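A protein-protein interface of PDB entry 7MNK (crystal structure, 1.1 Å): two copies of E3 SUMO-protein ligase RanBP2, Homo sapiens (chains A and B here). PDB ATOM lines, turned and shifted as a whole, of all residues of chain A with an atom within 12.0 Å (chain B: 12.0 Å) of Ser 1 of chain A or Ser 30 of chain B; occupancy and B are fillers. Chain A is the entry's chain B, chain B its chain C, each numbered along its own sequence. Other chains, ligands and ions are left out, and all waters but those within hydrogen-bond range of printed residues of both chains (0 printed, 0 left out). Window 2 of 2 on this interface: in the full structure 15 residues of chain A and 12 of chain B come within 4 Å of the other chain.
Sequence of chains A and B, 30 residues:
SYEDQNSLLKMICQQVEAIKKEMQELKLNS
Of the 11 printed residues of chain A, 6 touch a printed residue of chain B. Hydrophobic or aromatic side chains of chain A within 4 Å of the printed part of chain B: Tyr 2, Leu 8, Leu 9 and Ile 12. Of the 10 printed residues of chain B, 7 touch a printed residue of chain A. Among the printed residues, 13 pairs touch across the chains. Among the printed residues, no Asp or Glu carboxylate lies within 4 Å of a Lys or Arg side-chain nitrogen of the other chain.
Ser 30 of chain B touches Ser 1 of chain A (OXT to CA, 3.4 Å). Tyr 2 of chain A touches Lys 27 of chain B (OH to CD, 3.6 Å). CZ of Tyr 2 of chain A touches CB of Ser 30 of chain B, at 3.5 Å. Gln 5 of chain A touches Asn 29 of chain B. Gln 5 of chain A touches Ser 30 of chain B. O of Glu 22 of chain B touches CD2 of Leu 8 of chain A, at 3.9 Å. Leu 8 of chain A touches Leu 26 of chain B (CD2 to N, 3.7 Å). Leu 9 of chain A touches Leu 26 of chain B. O of Glu 22 of chain B touches CD1 of Ile 12 of chain A, 3.8 Å away. Ile 12 of chain A touches Met 23 of chain B.
Printed residues of chain B within 4 Å of Ser 1 of chain A: Asn 29 (2.9 Å) and Ser 30 (3.4 Å). Of the printed residues of chain B, Tyr 2 of chain A touches Lys 27 (3.6 Å) and Ser 30 (3.5 Å). Asp 4 of chain A touches none of the printed residues of chain B. Of the printed residues of chain B, Gln 5 of chain A touches Leu 26, Asn 29 and Ser 30. Printed residues of chain A within 4 Å of Glu 22 of chain B: Leu 8 and Ile 12. Leu 26 of chain B touches three residues of chain A. Lys 27 of chain B touches one residue of chain A. Of the printed residues of chain A, Ser 30 of chain B touches Ser 1, Tyr 2 and Gln 5. The nearest printed residue of chain B that does not touch Ser 1 of chain A is Leu 26 of chain B (5.4 Å). The nearest printed residue of chain A that does not touch Ser 30 of chain B is Asp 4 of chain A (6.4 Å). The nearest printed residue of chain B that does not touch Leu 9 of chain A is Glu 22 of chain B (7.3 Å).
N of Ser 1 of chain A sits at hydrogen-bond distance from O of Asn 29 of chain B (2.9 Å). O of Leu 26 of chain B lies within hydrogen-bond range of NE2 of Gln 5 of chain A (3.1 Å).
No position is printed for both chains.
The backbone carbonyl oxygen (O) of Glu 25 of chain B is in hydrogen-bond range of the side-chain amide nitrogen (ND2) of Asn 29 of chain B, at 3.1 Å. N of Glu 3 of chain A sits at hydrogen-bond distance from OG of Ser 1 of chain A. The side-chain amide nitrogen (NE2) of Gln 5 of chain A lies within hydrogen-bond range of the backbone carbonyl oxygen (O) of Ser 1 of chain A (3.0 Å). OD1 of Asp 4 of chain A is in hydrogen-bond range of N of Ser 1 of chain A (3.1 Å). O of Lys 27 of chain B is in hydrogen-bond range of OG of Ser 30 of chain B (2.8 Å).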
ATOM      1  N   SER A   1     -23.890 -27.593  10.451  1.00  0.00           N
ATOM      2  CA  SER A   1     -23.127 -26.669   9.577  1.00  0.00           C
ATOM      3  C   SER A   1     -22.622 -25.518  10.419  1.00  0.00           C
ATOM      4  O   SER A   1     -22.911 -25.489  11.614  1.00  0.00           O
ATOM      5  CB  SER A   1     -24.004 -26.173   8.445  1.00  0.00           C
ATOM      6  OG  SER A   1     -25.069 -25.433   8.994  1.00  0.00           O
ATOM      7  N   TYR A   2     -21.938 -24.523   9.798  1.00  0.00           N
ATOM      8  CA  TYR A   2     -21.652 -23.275  10.489  1.00  0.00           C
ATOM      9  C   TYR A   2     -22.849 -22.357  10.474  1.00  0.00           C
ATOM     10  O   TYR A   2     -22.786 -21.298  11.099  1.00  0.00           O
ATOM     11  CB  TYR A   2     -20.461 -22.520   9.899  1.00  0.00           C
ATOM     12  CG  TYR A   2     -19.147 -23.111  10.282  1.00  0.00           C
ATOM     13  CD1 TYR A   2     -18.680 -23.085  11.607  1.00  0.00           C
ATOM     14  CD2 TYR A   2     -18.372 -23.720   9.319  1.00  0.00           C
ATOM     15  CE1 TYR A   2     -17.443 -23.655  11.956  1.00  0.00           C
ATOM     16  CE2 TYR A   2     -17.126 -24.268   9.636  1.00  0.00           C
ATOM     17  CZ  TYR A   2     -16.671 -24.253  10.972  1.00  0.00           C
ATOM     18  OH  TYR A   2     -15.451 -24.834  11.300  1.00  0.00           O
ATOM     19  N   GLU A   3     -23.932 -22.729   9.761  1.00  0.00           N
ATOM     20  CA  GLU A   3     -25.105 -21.877   9.606  1.00  0.00           C
ATOM     21  C   GLU A   3     -26.280 -22.237  10.506  1.00  0.00           C
ATOM     22  O   GLU A   3     -27.282 -21.523  10.478  1.00  0.00           O
ATOM     23  CB  GLU A   3     -25.589 -21.897   8.138  1.00  0.00           C
ATOM     24  CG  GLU A   3     -24.518 -21.525   7.118  1.00  0.00           C
ATOM     25  CD  GLU A   3     -25.074 -21.352   5.710  1.00  0.00           C
ATOM     26  OE1 GLU A   3     -26.299 -21.530   5.522  1.00  0.00           O
ATOM     27  OE2 GLU A   3     -24.290 -21.033   4.798  1.00  0.00           O
ATOM     28  N   ASP A   4     -26.196 -23.325  11.287  1.00  0.00           N
ATOM     29  CA  ASP A   4     -27.316 -23.747  12.128  1.00  0.00           C
ATOM     30  C   ASP A   4     -26.974 -23.809  13.605  1.00  0.00           C
ATOM     31  O   ASP A   4     -27.703 -24.434  14.375  1.00  0.00           O
ATOM     32  CB  ASP A   4     -27.993 -25.034  11.644  1.00  0.00           C
ATOM     33  CG  ASP A   4     -27.159 -26.280  11.829  1.00  0.00           C
ATOM     34  OD1 ASP A   4     -25.987 -26.186  12.241  1.00  0.00           O
ATOM     35  OD2 ASP A   4     -27.687 -27.386  11.537  1.00  0.00           O
ATOM     36  N   GLN A   5     -25.903 -23.119  14.022  1.00  0.00           N
ATOM     37  CA  GLN A   5     -25.373 -23.237  15.374  1.00  0.00           C
ATOM     38  C   GLN A   5     -25.289 -21.906  16.104  1.00  0.00           C
ATOM     39  O   GLN A   5     -24.423 -21.706  16.967  1.00  0.00           O
ATOM     40  CB  GLN A   5     -24.020 -23.943  15.402  1.00  0.00           C
ATOM     41  CG  GLN A   5     -24.081 -25.366  14.884  1.00  0.00           C
ATOM     42  CD  GLN A   5     -22.834 -26.100  15.255  1.00  0.00           C
ATOM     43  OE1 GLN A   5     -22.674 -26.540  16.403  1.00  0.00           O
ATOM     44  NE2 GLN A   5     -21.900 -26.197  14.328  1.00  0.00           N
ATOM     45  N   ASN A   6     -26.213 -21.000  15.840  1.00  0.00           N
ATOM     46  CA  ASN A   6     -26.105 -19.693  16.466  1.00  0.00           C
ATOM     47  C   ASN A   6     -26.133 -19.771  17.976  1.00  0.00           C
ATOM     48  O   ASN A   6     -25.403 -19.033  18.642  1.00  0.00           O
ATOM     49  CB  ASN A   6     -27.177 -18.720  15.971  1.00  0.00           C
ATOM     50  CG  ASN A   6     -26.837 -17.311  16.377  1.00  0.00           C
ATOM     51  OD1 ASN A   6     -25.807 -16.769  15.944  1.00  0.00           O
ATOM     52  ND2 ASN A   6     -27.646 -16.724  17.217  1.00  0.00           N
ATOM     53  N   SER A   7     -26.988 -20.633  18.535  1.00  0.00           N
ATOM     54  CA  SER A   7     -27.117 -20.724  19.991  1.00  0.00           C
ATOM     55  C   SER A   7     -25.786 -21.097  20.644  1.00  0.00           C
ATOM     56  O   SER A   7     -25.389 -20.508  21.651  1.00  0.00           O
ATOM     57  CB  SER A   7     -28.212 -21.734  20.347  1.00  0.00           C
ATOM     58  OG  SER A   7     -28.323 -21.939  21.744  1.00  0.00           O
ATOM     59  N   LEU A   8     -25.087 -22.073  20.079  1.00  0.00           N
ATOM     60  CA  LEU A   8     -23.803 -22.509  20.629  1.00  0.00           C
ATOM     61  C   LEU A   8     -22.738 -21.434  20.432  1.00  0.00           C
ATOM     62  O   LEU A   8     -21.948 -21.176  21.343  1.00  0.00           O
ATOM     63  CB  LEU A   8     -23.384 -23.836  19.999  1.00  0.00           C
ATOM     64  CG  LEU A   8     -22.030 -24.385  20.463  1.00  0.00           C
ATOM     65  CD1 LEU A   8     -21.972 -24.588  21.970  1.00  0.00           C
ATOM     66  CD2 LEU A   8     -21.735 -25.686  19.744  1.00  0.00           C
ATOM     67  N   LEU A   9     -22.720 -20.780  19.277  1.00  0.00           N
ATOM     68  CA  LEU A   9     -21.814 -19.666  19.077  1.00  0.00           C
ATOM     69  C   LEU A   9     -22.023 -18.585  20.134  1.00  0.00           C
ATOM     70  O   LEU A   9     -21.052 -18.037  20.677  1.00  0.00           O
ATOM     71  CB  LEU A   9     -21.974 -19.108  17.663  1.00  0.00           C
ATOM     72  CG  LEU A   9     -21.386 -19.979  16.545  1.00  0.00           C
ATOM     73  CD1 LEU A   9     -22.016 -19.638  15.196  1.00  0.00           C
ATOM     74  CD2 LEU A   9     -19.883 -19.831  16.469  1.00  0.00           C
ATOM     75  N   LYS A  10     -23.271 -18.250  20.406  1.00  0.00           N
ATOM     76  CA  LYS A  10     -23.601 -17.238  21.392  1.00  0.00           C
ATOM     77  C   LYS A  10     -23.110 -17.657  22.771  1.00  0.00           C
ATOM     78  O   LYS A  10     -22.518 -16.858  23.499  1.00  0.00           O
ATOM     79  CB  LYS A  10     -25.096 -16.990  21.394  1.00  0.00           C
ATOM     80  CG  LYS A  10     -25.530 -15.933  22.386  1.00  0.00           C
ATOM     81  CD  LYS A  10     -27.027 -15.692  22.308  1.00  0.00           C
ATOM     82  CE  LYS A  10     -27.438 -14.558  23.195  1.00  0.00           C
ATOM     83  NZ  LYS A  10     -28.834 -14.140  22.862  1.00  0.00           N
ATOM     84  N   ILE A  12     -20.636 -19.704  23.544  1.00  0.00           N
ATOM     85  CA  ILE A  12     -19.184 -19.608  23.579  1.00  0.00           C
ATOM     86  C   ILE A  12     -18.748 -18.167  23.742  1.00  0.00           C
ATOM     87  O   ILE A  12     -17.870 -17.853  24.557  1.00  0.00           O
ATOM     88  CB  ILE A  12     -18.542 -20.264  22.334  1.00  0.00           C
ATOM     89  CG1 ILE A  12     -18.807 -21.762  22.334  1.00  0.00           C
ATOM     90  CG2 ILE A  12     -17.042 -19.998  22.335  1.00  0.00           C
ATOM     91  CD1 ILE A  12     -18.560 -22.421  20.971  1.00  0.00           C
ATOM     92  N   LYS B  21     -14.346 -27.701  25.218  1.00  0.00           N
ATOM     93  CA  LYS B  21     -15.277 -28.749  24.821  1.00  0.00           C
ATOM     94  C   LYS B  21     -16.367 -28.225  23.904  1.00  0.00           C
ATOM     95  O   LYS B  21     -16.793 -28.919  22.987  1.00  0.00           O
ATOM     96  CB  LYS B  21     -15.883 -29.377  26.071  1.00  0.00           C
ATOM     97  CG  LYS B  21     -14.883 -30.194  26.856  1.00  0.00           C
ATOM     98  CD  LYS B  21     -15.536 -30.934  27.989  1.00  0.00           C
ATOM     99  CE  LYS B  21     -14.553 -31.891  28.654  1.00  0.00           C
ATOM    100  NZ  LYS B  21     -14.563 -31.791  30.139  1.00  0.00           N
ATOM    101  N   GLU B  22     -16.845 -27.016  24.149  1.00  0.00           N
ATOM    102  CA  GLU B  22     -17.898 -26.434  23.328  1.00  0.00           C
ATOM    103  C   GLU B  22     -17.394 -26.044  21.944  1.00  0.00           C
ATOM    104  O   GLU B  22     -18.114 -26.213  20.951  1.00  0.00           O
ATOM    105  CB  GLU B  22     -18.514 -25.234  24.043  1.00  0.00           C
ATOM    106  CG  GLU B  22     -19.331 -25.694  25.249  1.00  0.00           C
ATOM    107  CD  GLU B  22     -19.333 -24.735  26.409  1.00  0.00           C
ATOM    108  OE1 GLU B  22     -19.031 -23.518  26.188  1.00  0.00           O
ATOM    109  OE2 GLU B  22     -19.570 -25.169  27.566  1.00  0.00           O
ATOM    110  N   MET B  23     -16.166 -25.538  21.844  1.00  0.00           N
ATOM    111  CA  MET B  23     -15.569 -25.244  20.540  1.00  0.00           C
ATOM    112  C   MET B  23     -15.363 -26.517  19.743  1.00  0.00           C
ATOM    113  O   MET B  23     -15.554 -26.525  18.520  1.00  0.00           O
ATOM    114  CB  MET B  23     -14.259 -24.494  20.748  1.00  0.00           C
ATOM    115  CG  MET B  23     -14.488 -23.078  21.191  1.00  0.00           C
ATOM    116  SD  MET B  23     -12.898 -22.426  21.762  1.00  0.00           S
ATOM    117  CE  MET B  23     -13.406 -20.746  22.056  1.00  0.00           C
ATOM    118  N   GLN B  24     -14.993 -27.609  20.424  1.00  0.00           N
ATOM    119  CA  GLN B  24     -14.897 -28.891  19.739  1.00  0.00           C
ATOM    120  C   GLN B  24     -16.265 -29.354  19.265  1.00  0.00           C
ATOM    121  O   GLN B  24     -16.400 -29.825  18.131  1.00  0.00           O
ATOM    122  CB  GLN B  24     -14.260 -29.916  20.665  1.00  0.00           C
ATOM    123  CG  GLN B  24     -12.792 -29.658  20.867  1.00  0.00           C
ATOM    124  CD  GLN B  24     -12.170 -30.690  21.771  1.00  0.00           C
ATOM    125  OE1 GLN B  24     -12.830 -31.241  22.675  1.00  0.00           O
ATOM    126  NE2 GLN B  24     -10.892 -30.977  21.544  1.00  0.00           N
ATOM    127  N   GLU B  25     -17.292 -29.241  20.114  1.00  0.00           N
ATOM    128  CA  GLU B  25     -18.659 -29.590  19.720  1.00  0.00           C
ATOM    129  C   GLU B  25     -19.100 -28.810  18.490  1.00  0.00           C
ATOM    130  O   GLU B  25     -19.728 -29.367  17.580  1.00  0.00           O
ATOM    131  CB  GLU B  25     -19.568 -29.326  20.913  1.00  0.00           C
ATOM    132  CG  GLU B  25     -21.029 -29.589  20.717  1.00  0.00           C
ATOM    133  CD  GLU B  25     -21.835 -29.126  21.913  1.00  0.00           C
ATOM    134  OE1 GLU B  25     -21.517 -28.012  22.421  1.00  0.00           O
ATOM    135  OE2 GLU B  25     -22.737 -29.853  22.376  1.00  0.00           O
ATOM    136  N   LEU B  26     -18.790 -27.512  18.471  1.00  0.00           N
ATOM    137  CA  LEU B  26     -19.085 -26.644  17.342  1.00  0.00           C
ATOM    138  C   LEU B  26     -18.466 -27.180  16.077  1.00  0.00           C
ATOM    139  O   LEU B  26     -19.115 -27.256  15.032  1.00  0.00           O
ATOM    140  CB  LEU B  26     -18.615 -25.237  17.673  1.00  0.00           C
ATOM    141  CG  LEU B  26     -18.817 -24.174  16.621  1.00  0.00           C
ATOM    142  CD1 LEU B  26     -20.287 -23.768  16.487  1.00  0.00           C
ATOM    143  CD2 LEU B  26     -17.964 -22.915  16.957  1.00  0.00           C
ATOM    144  N   LYS B  27     -17.177 -27.537  16.141  1.00  0.00           N
ATOM    145  CA  LYS B  27     -16.491 -28.084  14.969  1.00  0.00           C
ATOM    146  C   LYS B  27     -17.060 -29.429  14.560  1.00  0.00           C
ATOM    147  O   LYS B  27     -17.229 -29.693  13.361  1.00  0.00           O
ATOM    148  CB  LYS B  27     -14.992 -28.191  15.260  1.00  0.00           C
ATOM    149  CG  LYS B  27     -14.138 -28.655  14.092  1.00  0.00           C
ATOM    150  CD  LYS B  27     -13.974 -27.556  13.042  1.00  0.00           C
ATOM    151  CE  LYS B  27     -12.752 -27.669  12.188  1.00  0.00           C
ATOM    152  NZ  LYS B  27     -13.080 -28.780  11.363  1.00  0.00           N
ATOM    153  N   LEU B  28     -17.333 -30.308  15.531  1.00  0.00           N
ATOM    154  CA  LEU B  28     -17.897 -31.617  15.207  1.00  0.00           C
ATOM    155  C   LEU B  28     -19.244 -31.509  14.501  1.00  0.00           C
ATOM    156  O   LEU B  28     -19.574 -32.343  13.650  1.00  0.00           O
ATOM    157  CB  LEU B  28     -18.028 -32.472  16.456  1.00  0.00           C
ATOM    158  CG  LEU B  28     -16.695 -32.926  17.069  1.00  0.00           C
ATOM    159  CD1 LEU B  28     -16.925 -33.631  18.394  1.00  0.00           C
ATOM    160  CD2 LEU B  28     -15.877 -33.822  16.135  1.00  0.00           C
ATOM    161  N   ASN B  29     -20.020 -30.468  14.807  1.00  0.00           N
ATOM    162  CA  ASN B  29     -21.307 -30.228  14.161  1.00  0.00           C
ATOM    163  C   ASN B  29     -21.229 -29.309  12.941  1.00  0.00           C
ATOM    164  O   ASN B  29     -22.260 -29.072  12.287  1.00  0.00           O
ATOM    165  CB  ASN B  29     -22.266 -29.601  15.179  1.00  0.00           C
ATOM    166  CG  ASN B  29     -22.604 -30.524  16.308  1.00  0.00           C
ATOM    167  OD1 ASN B  29     -22.759 -31.713  16.128  1.00  0.00           O
ATOM    168  ND2 ASN B  29     -22.737 -29.966  17.498  1.00  0.00           N
ATOM    169  N   SER B  30     -20.055 -28.789  12.616  1.00  0.00           N
ATOM    170  CA  SER B  30     -19.908 -27.870  11.495  1.00  0.00           C
ATOM    171  C   SER B  30     -19.969 -28.593  10.145  1.00  0.00           C
ATOM    172  O   SER B  30     -19.921 -29.822  10.042  1.00  0.00           O
ATOM    173  CB  SER B  30     -18.584 -27.115  11.581  1.00  0.00           C
ATOM    174  OG  SER B  30     -17.510 -27.970  11.222  1.00  0.00           O
ATOM    175  OXT SER B  30     -20.051 -27.929   9.107  1.00  0.00           O
